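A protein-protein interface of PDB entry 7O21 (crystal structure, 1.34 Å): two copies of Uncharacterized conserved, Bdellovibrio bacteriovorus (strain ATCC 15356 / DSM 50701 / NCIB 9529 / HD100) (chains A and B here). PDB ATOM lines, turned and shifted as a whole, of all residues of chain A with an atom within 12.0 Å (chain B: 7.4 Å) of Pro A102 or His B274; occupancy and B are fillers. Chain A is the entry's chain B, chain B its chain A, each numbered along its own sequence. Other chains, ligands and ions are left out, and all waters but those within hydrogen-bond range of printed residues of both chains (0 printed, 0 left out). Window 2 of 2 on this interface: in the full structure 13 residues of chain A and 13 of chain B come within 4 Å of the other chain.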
ATOM      1  N   ARG A  98      -9.187  38.762  -7.655  1.00  0.00           N
ATOM      2  CA  ARG A  98      -8.162  38.068  -6.886  1.00  0.00           C
ATOM      3  C   ARG A  98      -8.637  36.648  -6.584  1.00  0.00           C
ATOM      4  O   ARG A  98      -9.735  36.456  -6.048  1.00  0.00           O
ATOM      5  CB  ARG A  98      -7.881  38.818  -5.580  1.00  0.00           C
ATOM      6  CG  ARG A  98      -6.953  38.102  -4.616  1.00  0.00           C
ATOM      7  CD  ARG A  98      -6.712  38.967  -3.383  1.00  0.00           C
ATOM      8  NE  ARG A  98      -6.146  38.210  -2.272  1.00  0.00           N
ATOM      9  CZ  ARG A  98      -5.375  38.739  -1.329  1.00  0.00           C
ATOM     10  NH1 ARG A  98      -5.074  40.031  -1.360  1.00  0.00           N
ATOM     11  NH2 ARG A  98      -4.901  37.976  -0.353  1.00  0.00           N
ATOM     12  N   LEU A  99      -7.817  35.655  -6.940  1.00  0.00           N
ATOM     13  CA  LEU A  99      -8.148  34.239  -6.805  1.00  0.00           C
ATOM     14  C   LEU A  99      -7.128  33.545  -5.910  1.00  0.00           C
ATOM     15  O   LEU A  99      -5.950  33.915  -5.883  1.00  0.00           O
ATOM     16  CB  LEU A  99      -8.137  33.537  -8.171  1.00  0.00           C
ATOM     17  CG  LEU A  99      -8.970  34.201  -9.266  1.00  0.00           C
ATOM     18  CD1 LEU A  99      -8.837  33.440 -10.572  1.00  0.00           C
ATOM     19  CD2 LEU A  99     -10.425  34.314  -8.841  1.00  0.00           C
ATOM     20  N   SER A 100      -7.572  32.525  -5.183  1.00  0.00           N
ATOM     21  CA  SER A 100      -6.648  31.755  -4.353  1.00  0.00           C
ATOM     22  C   SER A 100      -7.210  30.353  -4.147  1.00  0.00           C
ATOM     23  O   SER A 100      -8.221  29.973  -4.747  1.00  0.00           O
ATOM     24  CB  SER A 100      -6.344  32.471  -3.032  1.00  0.00           C
ATOM     25  OG  SER A 100      -5.325  31.787  -2.315  1.00  0.00           O
ATOM     26  N   GLN A 101      -6.546  29.576  -3.301  1.00  0.00           N
ATOM     27  CA  GLN A 101      -7.053  28.260  -2.962  1.00  0.00           C
ATOM     28  C   GLN A 101      -8.337  28.418  -2.149  1.00  0.00           C
ATOM     29  O   GLN A 101      -8.487  29.382  -1.392  1.00  0.00           O
ATOM     30  CB  GLN A 101      -6.027  27.508  -2.122  1.00  0.00           C
ATOM     31  CG  GLN A 101      -4.862  26.927  -2.914  1.00  0.00           C
ATOM     32  CD  GLN A 101      -3.855  27.987  -3.322  1.00  0.00           C
ATOM     33  OE1 GLN A 101      -3.194  28.594  -2.477  1.00  0.00           O
ATOM     34  NE2 GLN A 101      -3.733  28.217  -4.628  1.00  0.00           N
ATOM     35  N   PRO A 102      -9.283  27.486  -2.287  1.00  0.00           N
ATOM     36  CA  PRO A 102      -9.215  26.246  -3.062  1.00  0.00           C
ATOM     37  C   PRO A 102      -9.724  26.383  -4.497  1.00  0.00           C
ATOM     38  O   PRO A 102      -9.819  25.378  -5.190  1.00  0.00           O
ATOM     39  CB  PRO A 102     -10.172  25.336  -2.296  1.00  0.00           C
ATOM     40  CG  PRO A 102     -11.234  26.274  -1.838  1.00  0.00           C
ATOM     41  CD  PRO A 102     -10.501  27.539  -1.459  1.00  0.00           C
ATOM     42  N   LYS A 103     -10.054  27.602  -4.940  1.00  0.00           N
ATOM     43  CA  LYS A 103     -10.597  27.753  -6.285  1.00  0.00           C
ATOM     44  C   LYS A 103      -9.550  27.449  -7.350  1.00  0.00           C
ATOM     45  O   LYS A 103      -9.875  26.911  -8.415  1.00  0.00           O
ATOM     46  CB  LYS A 103     -11.167  29.157  -6.462  1.00  0.00           C
ATOM     47  CG  LYS A 103     -12.233  29.522  -5.440  1.00  0.00           C
ATOM     48  CD  LYS A 103     -13.426  28.561  -5.487  1.00  0.00           C
ATOM     49  CE  LYS A 103     -14.487  28.964  -4.463  1.00  0.00           C
ATOM     50  NZ  LYS A 103     -15.493  27.878  -4.227  1.00  0.00           N
ATOM     51  N   ILE A 104      -8.299  27.827  -7.105  1.00  0.00           N
ATOM     52  CA  ILE A 104      -7.244  27.559  -8.079  1.00  0.00           C
ATOM     53  C   ILE A 104      -6.138  26.719  -7.451  1.00  0.00           C
ATOM     54  O   ILE A 104      -5.866  26.858  -6.251  1.00  0.00           O
ATOM     55  CB  ILE A 104      -6.712  28.858  -8.708  1.00  0.00           C
ATOM     56  CG1 ILE A 104      -6.203  29.797  -7.620  1.00  0.00           C
ATOM     57  CG2 ILE A 104      -7.809  29.501  -9.548  1.00  0.00           C
ATOM     58  CD1 ILE A 104      -5.420  30.989  -8.164  1.00  0.00           C
ATOM     59  N   PRO A 105      -5.491  25.844  -8.225  1.00  0.00           N
ATOM     60  CA  PRO A 105      -4.474  24.939  -7.671  1.00  0.00           C
ATOM     61  C   PRO A 105      -3.159  25.662  -7.407  1.00  0.00           C
ATOM     62  O   PRO A 105      -2.637  26.380  -8.270  1.00  0.00           O
ATOM     63  CB  PRO A 105      -4.305  23.884  -8.775  1.00  0.00           C
ATOM     64  CG  PRO A 105      -4.715  24.579 -10.026  1.00  0.00           C
ATOM     65  CD  PRO A 105      -5.810  25.533  -9.625  1.00  0.00           C
ATOM     66  N   PHE A 106      -2.617  25.454  -6.207  1.00  0.00           N
ATOM     67  CA  PHE A 106      -1.306  26.007  -5.881  1.00  0.00           C
ATOM     68  C   PHE A 106      -0.233  25.507  -6.844  1.00  0.00           C
ATOM     69  O   PHE A 106       0.719  26.242  -7.148  1.00  0.00           O
ATOM     70  CB  PHE A 106      -0.932  25.635  -4.440  1.00  0.00           C
ATOM     71  CG  PHE A 106       0.330  26.294  -3.941  1.00  0.00           C
ATOM     72  CD1 PHE A 106       1.572  25.691  -4.113  1.00  0.00           C
ATOM     73  CD2 PHE A 106       0.266  27.515  -3.293  1.00  0.00           C
ATOM     74  CE1 PHE A 106       2.735  26.310  -3.635  1.00  0.00           C
ATOM     75  CE2 PHE A 106       1.417  28.136  -2.821  1.00  0.00           C
ATOM     76  CZ  PHE A 106       2.648  27.531  -3.001  1.00  0.00           C
ATOM     77  N   SER A 107      -0.353  24.261  -7.315  1.00  0.00           N
ATOM     78  CA  SER A 107       0.684  23.683  -8.169  1.00  0.00           C
ATOM     79  C   SER A 107       0.849  24.455  -9.471  1.00  0.00           C
ATOM     80  O   SER A 107       1.931  24.446 -10.068  1.00  0.00           O
ATOM     81  CB  SER A 107       0.334  22.228  -8.477  1.00  0.00           C
ATOM     82  OG  SER A 107      -0.855  22.152  -9.242  1.00  0.00           O
ATOM     83  N   LEU A 108      -0.205  25.113  -9.938  1.00  0.00           N
ATOM     84  CA  LEU A 108      -0.145  25.900 -11.164  1.00  0.00           C
ATOM     85  C   LEU A 108      -0.032  27.395 -10.908  1.00  0.00           C
ATOM     86  O   LEU A 108       0.537  28.110 -11.739  1.00  0.00           O
ATOM     87  CB  LEU A 108      -1.389  25.660 -12.033  1.00  0.00           C
ATOM     88  CG  LEU A 108      -1.690  24.249 -12.542  1.00  0.00           C
ATOM     89  CD1 LEU A 108      -2.938  24.281 -13.419  1.00  0.00           C
ATOM     90  CD2 LEU A 108      -0.503  23.673 -13.303  1.00  0.00           C
ATOM     91  N   TYR A 109      -0.563  27.892  -9.787  1.00  0.00           N
ATOM     92  CA  TYR A 109      -0.748  29.321  -9.628  1.00  0.00           C
ATOM     93  C   TYR A 109      -0.129  29.886  -8.358  1.00  0.00           C
ATOM     94  O   TYR A 109      -0.196  31.108  -8.147  1.00  0.00           O
ATOM     95  CB  TYR A 109      -2.252  29.684  -9.716  1.00  0.00           C
ATOM     96  CG  TYR A 109      -2.852  29.269 -11.034  1.00  0.00           C
ATOM     97  CD1 TYR A 109      -2.428  29.860 -12.213  1.00  0.00           C
ATOM     98  CD2 TYR A 109      -3.803  28.248 -11.116  1.00  0.00           C
ATOM     99  CE1 TYR A 109      -2.939  29.480 -13.431  1.00  0.00           C
ATOM    100  CE2 TYR A 109      -4.315  27.851 -12.345  1.00  0.00           C
ATOM    101  CZ  TYR A 109      -3.886  28.480 -13.500  1.00  0.00           C
ATOM    102  OH  TYR A 109      -4.365  28.130 -14.734  1.00  0.00           O
ATOM    103  N   GLY A 110       0.467  29.049  -7.511  1.00  0.00           N
ATOM    104  CA  GLY A 110       0.929  29.590  -6.251  1.00  0.00           C
ATOM    105  C   GLY A 110      -0.248  30.040  -5.390  1.00  0.00           C
ATOM    106  O   GLY A 110      -1.384  29.593  -5.559  1.00  0.00           O
ATOM    107  N   ALA A 111       0.034  30.960  -4.466  1.00  0.00           N
ATOM    108  CA  ALA A 111      -0.956  31.332  -3.461  1.00  0.00           C
ATOM    109  C   ALA A 111      -2.019  32.290  -3.980  1.00  0.00           C
ATOM    110  O   ALA A 111      -3.080  32.415  -3.353  1.00  0.00           O
ATOM    111  CB  ALA A 111      -0.268  31.966  -2.249  1.00  0.00           C
ATOM    112  N   LEU A 112      -1.759  32.986  -5.085  1.00  0.00           N
ATOM    113  CA  LEU A 112      -2.654  34.038  -5.535  1.00  0.00           C
ATOM    114  C   LEU A 112      -2.528  34.192  -7.035  1.00  0.00           C
ATOM    115  O   LEU A 112      -1.438  34.069  -7.598  1.00  0.00           O
ATOM    116  CB  LEU A 112      -2.309  35.403  -4.926  1.00  0.00           C
ATOM    117  CG  LEU A 112      -2.621  35.671  -3.457  1.00  0.00           C
ATOM    118  CD1 LEU A 112      -2.077  37.029  -3.047  1.00  0.00           C
ATOM    119  CD2 LEU A 112      -4.126  35.610  -3.221  1.00  0.00           C
ATOM    120  N   ALA A 113      -3.655  34.495  -7.669  1.00  0.00           N
ATOM    121  CA  ALA A 113      -3.682  34.941  -9.049  1.00  0.00           C
ATOM    122  C   ALA A 113      -4.558  36.183  -9.137  1.00  0.00           C
ATOM    123  O   ALA A 113      -5.527  36.333  -8.389  1.00  0.00           O
ATOM    124  CB  ALA A 113      -4.251  33.858  -9.976  1.00  0.00           C
ATOM    125  N   TRP A 134      -3.338  36.228 -16.755  1.00  0.00           N
ATOM    126  CA  TRP A 134      -3.338  36.435 -15.320  1.00  0.00           C
ATOM    127  C   TRP A 134      -1.936  36.832 -14.880  1.00  0.00           C
ATOM    128  O   TRP A 134      -0.944  36.543 -15.558  1.00  0.00           O
ATOM    129  CB  TRP A 134      -3.667  35.134 -14.588  1.00  0.00           C
ATOM    130  CG  TRP A 134      -5.088  34.675 -14.675  1.00  0.00           C
ATOM    131  CD1 TRP A 134      -6.122  35.254 -15.371  1.00  0.00           C
ATOM    132  CD2 TRP A 134      -5.633  33.538 -14.011  1.00  0.00           C
ATOM    133  NE1 TRP A 134      -7.277  34.509 -15.193  1.00  0.00           N
ATOM    134  CE2 TRP A 134      -6.995  33.449 -14.368  1.00  0.00           C
ATOM    135  CE3 TRP A 134      -5.084  32.548 -13.185  1.00  0.00           C
ATOM    136  CZ2 TRP A 134      -7.827  32.433 -13.887  1.00  0.00           C
ATOM    137  CZ3 TRP A 134      -5.912  31.538 -12.715  1.00  0.00           C
ATOM    138  CH2 TRP A 134      -7.266  31.490 -13.061  1.00  0.00           C
ATOM    139  N   PHE B 226      -8.550  26.888 -16.368  1.00  0.00           N
ATOM    140  CA  PHE B 226      -8.727  25.444 -16.423  1.00  0.00           C
ATOM    141  C   PHE B 226      -9.127  24.974 -17.814  1.00  0.00           C
ATOM    142  O   PHE B 226      -9.791  25.684 -18.574  1.00  0.00           O
ATOM    143  CB  PHE B 226      -9.844  24.975 -15.480  1.00  0.00           C
ATOM    144  CG  PHE B 226      -9.543  25.169 -14.021  1.00  0.00           C
ATOM    145  CD1 PHE B 226      -8.807  24.228 -13.318  1.00  0.00           C
ATOM    146  CD2 PHE B 226     -10.032  26.274 -13.348  1.00  0.00           C
ATOM    147  CE1 PHE B 226      -8.536  24.387 -11.966  1.00  0.00           C
ATOM    148  CE2 PHE B 226      -9.777  26.445 -12.001  1.00  0.00           C
ATOM    149  CZ  PHE B 226      -9.027  25.497 -11.300  1.00  0.00           C
ATOM    150  N   HIS B 234      -7.458  18.975 -10.463  1.00  0.00           N
ATOM    151  CA  HIS B 234      -7.624  19.770  -9.259  1.00  0.00           C
ATOM    152  C   HIS B 234      -8.681  19.155  -8.345  1.00  0.00           C
ATOM    153  O   HIS B 234      -8.480  19.052  -7.126  1.00  0.00           O
ATOM    154  CB  HIS B 234      -7.979  21.194  -9.682  1.00  0.00           C
ATOM    155  CG  HIS B 234      -8.186  22.139  -8.552  1.00  0.00           C
ATOM    156  ND1 HIS B 234      -7.269  22.313  -7.537  1.00  0.00           N
ATOM    157  CD2 HIS B 234      -9.193  23.009  -8.304  1.00  0.00           C
ATOM    158  CE1 HIS B 234      -7.717  23.234  -6.702  1.00  0.00           C
ATOM    159  NE2 HIS B 234      -8.880  23.673  -7.143  1.00  0.00           N
ATOM    160  N   LYS B 235      -9.796  18.704  -8.918  1.00  0.00           N
ATOM    161  CA  LYS B 235     -10.825  18.065  -8.106  1.00  0.00           C
ATOM    162  C   LYS B 235     -10.303  16.803  -7.440  1.00  0.00           C
ATOM    163  O   LYS B 235     -10.625  16.528  -6.279  1.00  0.00           O
ATOM    164  CB  LYS B 235     -12.046  17.756  -8.959  1.00  0.00           C
ATOM    165  CG  LYS B 235     -12.748  19.019  -9.441  1.00  0.00           C
ATOM    166  CD  LYS B 235     -13.416  19.739  -8.281  1.00  0.00           C
ATOM    167  CE  LYS B 235     -14.354  20.829  -8.759  1.00  0.00           C
ATOM    168  NZ  LYS B 235     -13.678  22.150  -8.839  1.00  0.00           N
ATOM    169  N   LEU B 238      -7.969  17.886  -4.531  1.00  0.00           N
ATOM    170  CA  LEU B 238      -8.738  18.321  -3.371  1.00  0.00           C
ATOM    171  C   LEU B 238      -9.313  17.127  -2.629  1.00  0.00           C
ATOM    172  O   LEU B 238      -9.266  17.063  -1.394  1.00  0.00           O
ATOM    173  CB  LEU B 238      -9.862  19.263  -3.806  1.00  0.00           C
ATOM    174  CG  LEU B 238      -9.444  20.630  -4.327  1.00  0.00           C
ATOM    175  CD1 LEU B 238     -10.639  21.349  -4.940  1.00  0.00           C
ATOM    176  CD2 LEU B 238      -8.861  21.422  -3.179  1.00  0.00           C
ATOM    177  N   LYS B 241      -7.007  15.458  -0.238  1.00  0.00           N
ATOM    178  CA  LYS B 241      -6.671  16.215   0.961  1.00  0.00           C
ATOM    179  C   LYS B 241      -7.844  16.424   1.904  1.00  0.00           C
ATOM    180  O   LYS B 241      -7.639  16.493   3.121  1.00  0.00           O
ATOM    181  CB  LYS B 241      -6.087  17.581   0.586  1.00  0.00           C
ATOM    182  CG  LYS B 241      -4.842  17.498  -0.280  1.00  0.00           C
ATOM    183  CD  LYS B 241      -4.060  18.805  -0.269  1.00  0.00           C
ATOM    184  CE  LYS B 241      -4.673  19.843  -1.198  1.00  0.00           C
ATOM    185  NZ  LYS B 241      -4.328  21.229  -0.773  1.00  0.00           N
ATOM    186  N   TYR B 242      -9.064  16.529   1.381  1.00  0.00           N
ATOM    187  CA  TYR B 242     -10.244  16.854   2.180  1.00  0.00           C
ATOM    188  C   TYR B 242     -11.285  15.792   1.869  1.00  0.00           C
ATOM    189  O   TYR B 242     -11.952  15.860   0.831  1.00  0.00           O
ATOM    190  CB  TYR B 242     -10.750  18.251   1.840  1.00  0.00           C
ATOM    191  CG  TYR B 242      -9.696  19.305   2.059  1.00  0.00           C
ATOM    192  CD1 TYR B 242      -8.997  19.369   3.257  1.00  0.00           C
ATOM    193  CD2 TYR B 242      -9.369  20.211   1.058  1.00  0.00           C
ATOM    194  CE1 TYR B 242      -8.016  20.321   3.465  1.00  0.00           C
ATOM    195  CE2 TYR B 242      -8.386  21.168   1.256  1.00  0.00           C
ATOM    196  CZ  TYR B 242      -7.714  21.219   2.463  1.00  0.00           C
ATOM    197  OH  TYR B 242      -6.738  22.166   2.670  1.00  0.00           O
ATOM    198  N   LYS B 246     -19.188  19.561   1.651  1.00  0.00           N
ATOM    199  CA  LYS B 246     -20.612  19.855   1.578  1.00  0.00           C
ATOM    200  C   LYS B 246     -20.809  20.883   0.475  1.00  0.00           C
ATOM    201  O   LYS B 246     -20.103  21.894   0.442  1.00  0.00           O
ATOM    202  CB  LYS B 246     -21.099  20.461   2.897  1.00  0.00           C
ATOM    203  CG  LYS B 246     -21.244  19.469   4.051  1.00  0.00           C
ATOM    204  CD  LYS B 246     -21.049  20.183   5.385  1.00  0.00           C
ATOM    205  CE  LYS B 246     -22.296  20.158   6.247  1.00  0.00           C
ATOM    206  NZ  LYS B 246     -23.184  21.325   5.976  1.00  0.00           N
ATOM    207  N   ARG B 268     -22.949  27.325  -1.623  1.00  0.00           N
ATOM    208  CA  ARG B 268     -22.144  27.246  -0.412  1.00  0.00           C
ATOM    209  C   ARG B 268     -21.276  25.999  -0.518  1.00  0.00           C
ATOM    210  O   ARG B 268     -21.796  24.895  -0.702  1.00  0.00           O
ATOM    211  CB  ARG B 268     -23.038  27.161   0.820  1.00  0.00           C
ATOM    212  CG  ARG B 268     -22.269  27.194   2.135  1.00  0.00           C
ATOM    213  CD  ARG B 268     -23.210  26.940   3.303  1.00  0.00           C
ATOM    214  NE  ARG B 268     -22.539  27.140   4.588  1.00  0.00           N
ATOM    215  CZ  ARG B 268     -21.878  26.189   5.238  1.00  0.00           C
ATOM    216  NH1 ARG B 268     -21.796  24.971   4.721  1.00  0.00           N
ATOM    217  NH2 ARG B 268     -21.305  26.458   6.408  1.00  0.00           N
ATOM    218  N   TYR B 269     -19.963  26.185  -0.424  1.00  0.00           N
ATOM    219  CA  TYR B 269     -18.986  25.100  -0.466  1.00  0.00           C
ATOM    220  C   TYR B 269     -18.276  25.028   0.878  1.00  0.00           C
ATOM    221  O   TYR B 269     -17.767  26.042   1.365  1.00  0.00           O
ATOM    222  CB  TYR B 269     -17.936  25.379  -1.549  1.00  0.00           C
ATOM    223  CG  TYR B 269     -16.925  24.263  -1.713  1.00  0.00           C
ATOM    224  CD1 TYR B 269     -15.754  24.243  -0.973  1.00  0.00           C
ATOM    225  CD2 TYR B 269     -17.153  23.240  -2.617  1.00  0.00           C
ATOM    226  CE1 TYR B 269     -14.837  23.215  -1.128  1.00  0.00           C
ATOM    227  CE2 TYR B 269     -16.248  22.228  -2.789  1.00  0.00           C
ATOM    228  CZ  TYR B 269     -15.105  22.212  -2.033  1.00  0.00           C
ATOM    229  OH  TYR B 269     -14.210  21.193  -2.229  1.00  0.00           O
ATOM    230  N   GLU B 270     -18.214  23.835   1.457  1.00  0.00           N
ATOM    231  CA  GLU B 270     -17.559  23.654   2.750  1.00  0.00           C
ATOM    232  C   GLU B 270     -16.657  22.433   2.738  1.00  0.00           C
ATOM    233  O   GLU B 270     -17.092  21.337   2.381  1.00  0.00           O
ATOM    234  CB  GLU B 270     -18.577  23.496   3.882  1.00  0.00           C
ATOM    235  CG  GLU B 270     -17.907  23.234   5.238  1.00  0.00           C
ATOM    236  CD  GLU B 270     -18.839  23.430   6.425  1.00  0.00           C
ATOM    237  OE1 GLU B 270     -20.071  23.391   6.241  1.00  0.00           O
ATOM    238  OE2 GLU B 270     -18.337  23.614   7.553  1.00  0.00           O
ATOM    239  N   SER B 271     -15.419  22.627   3.167  1.00  0.00           N
ATOM    240  CA  SER B 271     -14.552  21.542   3.593  1.00  0.00           C
ATOM    241  C   SER B 271     -14.149  21.808   5.038  1.00  0.00           C
ATOM    242  O   SER B 271     -14.504  22.832   5.629  1.00  0.00           O
ATOM    243  CB  SER B 271     -13.304  21.471   2.721  1.00  0.00           C
ATOM    244  OG  SER B 271     -12.480  22.589   3.002  1.00  0.00           O
ATOM    245  N   ASP B 272     -13.369  20.894   5.609  1.00  0.00           N
ATOM    246  CA  ASP B 272     -12.923  21.127   6.978  1.00  0.00           C
ATOM    247  C   ASP B 272     -12.051  22.369   7.105  1.00  0.00           C
ATOM    248  O   ASP B 272     -11.909  22.901   8.211  1.00  0.00           O
ATOM    249  CB  ASP B 272     -12.220  19.889   7.530  1.00  0.00           C
ATOM    250  CG  ASP B 272     -13.208  18.842   8.006  1.00  0.00           C
ATOM    251  OD1 ASP B 272     -14.261  19.243   8.554  1.00  0.00           O
ATOM    252  OD2 ASP B 272     -12.950  17.639   7.819  1.00  0.00           O
ATOM    253  N   LYS B 273     -11.484  22.855   6.002  1.00  0.00           N
ATOM    254  CA  LYS B 273     -10.603  24.016   6.030  1.00  0.00           C
ATOM    255  C   LYS B 273     -11.345  25.342   5.869  1.00  0.00           C
ATOM    256  O   LYS B 273     -11.112  26.276   6.643  1.00  0.00           O
ATOM    257  CB  LYS B 273      -9.516  23.892   4.962  1.00  0.00           C
ATOM    258  CG  LYS B 273      -8.478  25.016   5.002  1.00  0.00           C
ATOM    259  CD  LYS B 273      -7.140  24.550   4.458  1.00  0.00           C
ATOM    260  CE  LYS B 273      -6.045  25.557   4.755  1.00  0.00           C
ATOM    261  NZ  LYS B 273      -5.853  25.712   6.222  1.00  0.00           N
ATOM    262  N   HIS B 274     -12.210  25.467   4.861  1.00  0.00           N
ATOM    263  CA  HIS B 274     -12.895  26.736   4.638  1.00  0.00           C
ATOM    264  C   HIS B 274     -14.332  26.522   4.177  1.00  0.00           C
ATOM    265  O   HIS B 274     -14.720  25.443   3.721  1.00  0.00           O
ATOM    266  CB  HIS B 274     -12.173  27.683   3.656  1.00  0.00           C
ATOM    267  CG  HIS B 274     -11.033  27.061   2.905  1.00  0.00           C
ATOM    268  ND1 HIS B 274     -11.196  25.996   2.046  1.00  0.00           N
ATOM    269  CD2 HIS B 274      -9.722  27.392   2.848  1.00  0.00           C
ATOM    270  CE1 HIS B 274     -10.029  25.682   1.513  1.00  0.00           C
ATOM    271  NE2 HIS B 274      -9.117  26.514   1.984  1.00  0.00           N
ATOM    272  N   VAL B 275     -15.113  27.589   4.325  1.00  0.00           N
ATOM    273  CA  VAL B 275     -16.458  27.708   3.778  1.00  0.00           C
ATOM    274  C   VAL B 275     -16.447  28.936   2.883  1.00  0.00           C
ATOM    275  O   VAL B 275     -15.887  29.975   3.244  1.00  0.00           O
ATOM    276  CB  VAL B 275     -17.509  27.891   4.892  1.00  0.00           C
ATOM    277  CG1 VAL B 275     -18.892  28.143   4.282  1.00  0.00           C
ATOM    278  CG2 VAL B 275     -17.537  26.677   5.812  1.00  0.00           C
ATOM    279  N   ASP B 276     -17.042  28.817   1.704  1.00  0.00           N
ATOM    280  CA  ASP B 276     -17.236  29.997   0.878  1.00  0.00           C
ATOM    281  C   ASP B 276     -18.616  29.987   0.232  1.00  0.00           C
ATOM    282  O   ASP B 276     -19.233  28.935   0.036  1.00  0.00           O
ATOM    283  CB  ASP B 276     -16.116  30.222  -0.163  1.00  0.00           C
ATOM    284  CG  ASP B 276     -15.932  29.050  -1.088  1.00  0.00           C
ATOM    285  OD1 ASP B 276     -16.863  28.741  -1.860  1.00  0.00           O
ATOM    286  OD2 ASP B 276     -14.840  28.448  -1.072  1.00  0.00           O
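The side-chain amino group (NZ) of Lys A103 lies within salt-bridge range of the side-chain carboxylate (OD1) of Asp B276 (2.9 Å). A ring nitrogen (NE2) of His B234 sits at hydrogen-bond distance from the backbone carbonyl oxygen (O) of Pro A102 (2.8 Å).
The side-chain hydroxyl of Ser B271 lies within hydrogen-bond range of the backbone NH of His B274, at 3.4 Å. N of Tyr B269 is in hydrogen-bond range of O of Asp B276 (2.9 Å). The backbone carbonyl oxygen of Ile A104 is in hydrogen-bond range of the side-chain amide nitrogen of Gln A101 (3.0 Å).
Pro A102 touches His B274. Lys A103 touches Phe B226. O of Lys A103 touches NE2 of His B234, 3.6 Å away. CE1 of His B234 touches C of Ile A104, at 3.9 Å. Phe B226 touches Pro A105 (CZ to CD, 3.6 Å). Pro A105 touches His B234.
Of the printed residues of chain B, Pro A102 touches His B234 (2.8 Å) and His B274 (3.5 Å). Printed residues of chain A within 4 Å of His B274: Pro A102 (3.5 Å). No residue of chain A comes within 4 Å of Tyr B269. Glu B270 touches none of the printed residues of chain A. Ser B271 touches none of the printed residues of chain A. No residue of chain A comes within 4 Å of Lys B273. No residue of chain A comes within 4 Å of Val B275. Of chain A, only Lys A103 (2.9 Å) comes within 4 Å of Asp B276. Printed residues of chain B within 4 Å of Ile A104: His B234 (3.9 Å). Of the printed residues of chain B, Pro A105 touches Phe B226 and His B234. Of the printed residues of chain B, Lys A103 touches Phe B226, His B234 and Asp B276. Of the printed residues of chain A, Phe B226 touches Lys A103 and Pro A105. Arg B268 touches none of the printed residues of chain A. The nearest printed residue of chain B that does not touch Pro A102 is Leu B238 (4.1 Å). The nearest printed residue of chain A that does not touch His B274 is Gln A101 (4.5 Å). The nearest printed residue of chain B that does not touch Lys A103 is Tyr B269 (4.4 Å).
Hydrophobic or aromatic side chains of chain B that line the printed part of chain A: Phe B226, His B234 and His B274. Of the 17 printed residues of chain A, 4 touch a printed residue of chain B. Printed residues of chain A that touch a printed residue of chain B: Pro A102, Lys A103, Ile A104 and Pro A105. Among the printed residues, 8 pairs touch across the chains. Among the printed residues, Asp or Glu carboxylates within 4 Å of a Lys or Arg side-chain nitrogen of the other chain: Lys A103 with Asp B276 (2.9 Å).
No position is printed for both chains.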
